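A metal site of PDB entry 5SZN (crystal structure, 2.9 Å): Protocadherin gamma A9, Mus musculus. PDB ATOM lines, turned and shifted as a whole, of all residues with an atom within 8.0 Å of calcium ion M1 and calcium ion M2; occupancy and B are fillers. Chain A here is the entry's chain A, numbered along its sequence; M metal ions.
OE2 of Glu 435 lies close to N of Gln 527.
The backbone carbonyl oxygen of Glu 435 sits at hydrogen-bond distance from the backbone NH of Phe 492 (3.4 Å).
The backbone NH (N) of Glu 435 lies within hydrogen-bond range of the backbone carbonyl oxygen (O) of Leu 525.
Residues that only touch calcium ion M1: Asp 526 (3.6 Å).
Of the 14 residues printed, 5 come within 4 Å of calcium ion M1.
The nearest printed residue that does not touch calcium ion M1 is Tyr 494 (4.2 Å).
Three residues have an atom within 4 Å of calcium ion M2: Glu 435, Asp 493 and Asp 529.
Along chain A the residues within 4 Å of calcium ion M2 span positions 435 to 529.
The side-chain carboxylate (OE1) of Glu 495 is bound to calcium ion M1 (2.4 Å).
Calcium ion M1 is bound by the side-chain carboxylate (OE2) of Glu 435 (2.5 Å).
Calcium ion M1 is bound by OD1 of Asp 529, at 2.5 Å.
OD2 of Asp 529 is bound to calcium ion M1 (2.5 Å).
OE2 of Glu 495 is bound to calcium ion M1 (2.6 Å).
Slightly farther from calcium ion M1 lies the side-chain carboxylate (OE1) of Glu 435 (2.9 Å).
Calcium ion M2 is bound by the side-chain carboxylate of Glu 435 (2.5 Å) and the side-chain carboxylate of Asp 493 (2.6 Å).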
ATOM      1  N   GLU A 435      -8.668  15.780   2.427  1.00  0.00           N
ATOM      2  CA  GLU A 435      -9.251  14.599   3.061  1.00  0.00           C
ATOM      3  C   GLU A 435      -8.297  13.970   4.064  1.00  0.00           C
ATOM      4  O   GLU A 435      -8.601  13.855   5.259  1.00  0.00           O
ATOM      5  CB  GLU A 435      -9.666  13.583   2.000  1.00  0.00           C
ATOM      6  CG  GLU A 435     -10.811  14.038   1.114  1.00  0.00           C
ATOM      7  CD  GLU A 435     -11.009  13.114  -0.066  1.00  0.00           C
ATOM      8  OE1 GLU A 435     -10.489  11.984  -0.023  1.00  0.00           O
ATOM      9  OE2 GLU A 435     -11.688  13.530  -1.031  1.00  0.00           O
ATOM     10  N   ASN A 436      -7.112  13.559   3.596  1.00  0.00           N
ATOM     11  CA  ASN A 436      -6.136  12.911   4.462  1.00  0.00           C
ATOM     12  C   ASN A 436      -5.865  13.773   5.686  1.00  0.00           C
ATOM     13  O   ASN A 436      -5.578  14.970   5.581  1.00  0.00           O
ATOM     14  CB  ASN A 436      -4.842  12.641   3.691  1.00  0.00           C
ATOM     15  CG  ASN A 436      -4.152  13.907   3.233  1.00  0.00           C
ATOM     16  OD1 ASN A 436      -4.795  14.901   2.903  1.00  0.00           O
ATOM     17  ND2 ASN A 436      -2.815  13.878   3.204  1.00  0.00           N
ATOM     18  N   SER A 491      -9.242  11.117  10.851  1.00  0.00           N
ATOM     19  CA  SER A 491      -9.103  11.474   9.454  1.00  0.00           C
ATOM     20  C   SER A 491     -10.477  11.807   8.869  1.00  0.00           C
ATOM     21  O   SER A 491     -11.521  11.407   9.391  1.00  0.00           O
ATOM     22  CB  SER A 491      -8.449  10.344   8.666  1.00  0.00           C
ATOM     23  OG  SER A 491      -7.929  10.832   7.433  1.00  0.00           O
ATOM     24  N   PHE A 492     -10.463  12.565   7.779  1.00  0.00           N
ATOM     25  CA  PHE A 492     -11.680  13.107   7.187  1.00  0.00           C
ATOM     26  C   PHE A 492     -11.845  12.584   5.768  1.00  0.00           C
ATOM     27  O   PHE A 492     -10.891  12.554   4.988  1.00  0.00           O
ATOM     28  CB  PHE A 492     -11.649  14.642   7.187  1.00  0.00           C
ATOM     29  N   ASP A 493     -13.073  12.174   5.441  1.00  0.00           N
ATOM     30  CA  ASP A 493     -13.436  11.810   4.076  1.00  0.00           C
ATOM     31  C   ASP A 493     -14.467  12.811   3.588  1.00  0.00           C
ATOM     32  O   ASP A 493     -15.459  13.081   4.284  1.00  0.00           O
ATOM     33  CB  ASP A 493     -13.981  10.383   4.006  1.00  0.00           C
ATOM     34  CG  ASP A 493     -13.526   9.645   2.772  1.00  0.00           C
ATOM     35  OD1 ASP A 493     -13.157  10.307   1.776  1.00  0.00           O
ATOM     36  OD2 ASP A 493     -13.531   8.395   2.788  1.00  0.00           O
ATOM     37  N   TYR A 494     -14.239  13.376   2.397  1.00  0.00           N
ATOM     38  CA  TYR A 494     -15.163  14.349   1.851  1.00  0.00           C
ATOM     39  C   TYR A 494     -16.555  13.760   1.631  1.00  0.00           C
ATOM     40  O   TYR A 494     -17.525  14.514   1.489  1.00  0.00           O
ATOM     41  CB  TYR A 494     -14.618  14.930   0.539  1.00  0.00           C
ATOM     42  CG  TYR A 494     -15.491  16.004  -0.069  1.00  0.00           C
ATOM     43  CD1 TYR A 494     -15.462  17.295   0.427  1.00  0.00           C
ATOM     44  CD2 TYR A 494     -16.330  15.719  -1.131  1.00  0.00           C
ATOM     45  CE1 TYR A 494     -16.260  18.290  -0.122  1.00  0.00           C
ATOM     46  CE2 TYR A 494     -17.132  16.706  -1.694  1.00  0.00           C
ATOM     47  CZ  TYR A 494     -17.091  17.985  -1.181  1.00  0.00           C
ATOM     48  OH  TYR A 494     -17.880  18.964  -1.737  1.00  0.00           O
ATOM     49  N   GLU A 495     -16.676  12.435   1.616  1.00  0.00           N
ATOM     50  CA  GLU A 495     -17.940  11.765   1.348  1.00  0.00           C
ATOM     51  C   GLU A 495     -18.779  11.532   2.592  1.00  0.00           C
ATOM     52  O   GLU A 495     -19.983  11.246   2.473  1.00  0.00           O
ATOM     53  CB  GLU A 495     -17.699  10.432   0.627  1.00  0.00           C
ATOM     54  CG  GLU A 495     -17.273  10.581  -0.827  1.00  0.00           C
ATOM     55  CD  GLU A 495     -15.887  11.183  -0.984  1.00  0.00           C
ATOM     56  OE1 GLU A 495     -15.099  11.124  -0.009  1.00  0.00           O
ATOM     57  OE2 GLU A 495     -15.582  11.715  -2.074  1.00  0.00           O
ATOM     58  N   GLN A 496     -18.195  11.623   3.791  1.00  0.00           N
ATOM     59  CA  GLN A 496     -18.979  11.610   5.013  1.00  0.00           C
ATOM     60  C   GLN A 496     -19.406  13.032   5.399  1.00  0.00           C
ATOM     61  O   GLN A 496     -20.602  13.336   5.416  1.00  0.00           O
ATOM     62  CB  GLN A 496     -18.186  10.961   6.148  1.00  0.00           C
ATOM     63  CG  GLN A 496     -18.970  10.752   7.439  1.00  0.00           C
ATOM     64  CD  GLN A 496     -20.025   9.663   7.334  1.00  0.00           C
ATOM     65  OE1 GLN A 496     -20.165   9.004   6.296  1.00  0.00           O
ATOM     66  NE2 GLN A 496     -20.780   9.467   8.414  1.00  0.00           N
ATOM     67  N   PHE A 497     -18.445  13.885   5.700  1.00  0.00           N
ATOM     68  CA  PHE A 497     -18.676  15.305   5.904  1.00  0.00           C
ATOM     69  C   PHE A 497     -17.988  16.098   4.804  1.00  0.00           C
ATOM     70  O   PHE A 497     -17.065  15.609   4.139  1.00  0.00           O
ATOM     71  CB  PHE A 497     -18.154  15.792   7.269  1.00  0.00           C
ATOM     72  CG  PHE A 497     -18.966  15.313   8.441  1.00  0.00           C
ATOM     73  CD1 PHE A 497     -20.126  14.580   8.263  1.00  0.00           C
ATOM     74  CD2 PHE A 497     -18.563  15.609   9.725  1.00  0.00           C
ATOM     75  CE1 PHE A 497     -20.864  14.139   9.348  1.00  0.00           C
ATOM     76  CE2 PHE A 497     -19.297  15.181  10.815  1.00  0.00           C
ATOM     77  CZ  PHE A 497     -20.443  14.448  10.628  1.00  0.00           C
ATOM     78  N   LEU A 525     -11.245  19.262   1.778  1.00  0.00           N
ATOM     79  CA  LEU A 525     -10.917  19.381   0.359  1.00  0.00           C
ATOM     80  C   LEU A 525     -10.849  18.004  -0.275  1.00  0.00           C
ATOM     81  O   LEU A 525     -10.322  17.061   0.319  1.00  0.00           O
ATOM     82  CB  LEU A 525      -9.580  20.114   0.168  1.00  0.00           C
ATOM     83  CG  LEU A 525      -9.513  21.528   0.741  1.00  0.00           C
ATOM     84  CD1 LEU A 525      -8.192  22.198   0.379  1.00  0.00           C
ATOM     85  CD2 LEU A 525     -10.695  22.364   0.247  1.00  0.00           C
ATOM     86  N   ASP A 526     -11.387  17.895  -1.489  1.00  0.00           N
ATOM     87  CA  ASP A 526     -11.482  16.619  -2.180  1.00  0.00           C
ATOM     88  C   ASP A 526     -10.167  16.293  -2.896  1.00  0.00           C
ATOM     89  O   ASP A 526      -9.461  17.178  -3.376  1.00  0.00           O
ATOM     90  CB  ASP A 526     -12.633  16.649  -3.184  1.00  0.00           C
ATOM     91  CG  ASP A 526     -12.891  15.299  -3.821  1.00  0.00           C
ATOM     92  OD1 ASP A 526     -13.664  14.506  -3.241  1.00  0.00           O
ATOM     93  OD2 ASP A 526     -12.325  15.029  -4.899  1.00  0.00           O
ATOM     94  N   GLN A 527      -9.857  14.995  -2.964  1.00  0.00           N
ATOM     95  CA  GLN A 527      -8.628  14.520  -3.577  1.00  0.00           C
ATOM     96  C   GLN A 527      -8.927  13.295  -4.436  1.00  0.00           C
ATOM     97  O   GLN A 527     -10.089  12.894  -4.601  1.00  0.00           O
ATOM     98  CB  GLN A 527      -7.578  14.195  -2.511  1.00  0.00           C
ATOM     99  N   ASN A 528      -7.875  12.698  -4.984  1.00  0.00           N
ATOM    100  CA  ASN A 528      -7.983  11.535  -5.856  1.00  0.00           C
ATOM    101  C   ASN A 528      -8.220  10.300  -5.000  1.00  0.00           C
ATOM    102  O   ASN A 528      -7.286   9.628  -4.563  1.00  0.00           O
ATOM    103  CB  ASN A 528      -6.739  11.383  -6.721  1.00  0.00           C
ATOM    104  N   ASP A 529      -9.498   9.992  -4.762  1.00  0.00           N
ATOM    105  CA  ASP A 529      -9.884   8.871  -3.912  1.00  0.00           C
ATOM    106  C   ASP A 529      -9.558   7.533  -4.564  1.00  0.00           C
ATOM    107  O   ASP A 529     -10.297   6.562  -4.407  1.00  0.00           O
ATOM    108  CB  ASP A 529     -11.379   8.956  -3.597  1.00  0.00           C
ATOM    109  CG  ASP A 529     -11.813  10.366  -3.250  1.00  0.00           C
ATOM    110  OD1 ASP A 529     -11.035  11.092  -2.603  1.00  0.00           O
ATOM    111  OD2 ASP A 529     -12.935  10.749  -3.641  1.00  0.00           O
HETATM  112 CA    CA M   1     -13.091  11.495  -1.266  1.00  0.00          CA
HETATM  113 CA    CA M   2     -11.190   9.601   0.258  1.00  0.00          CA
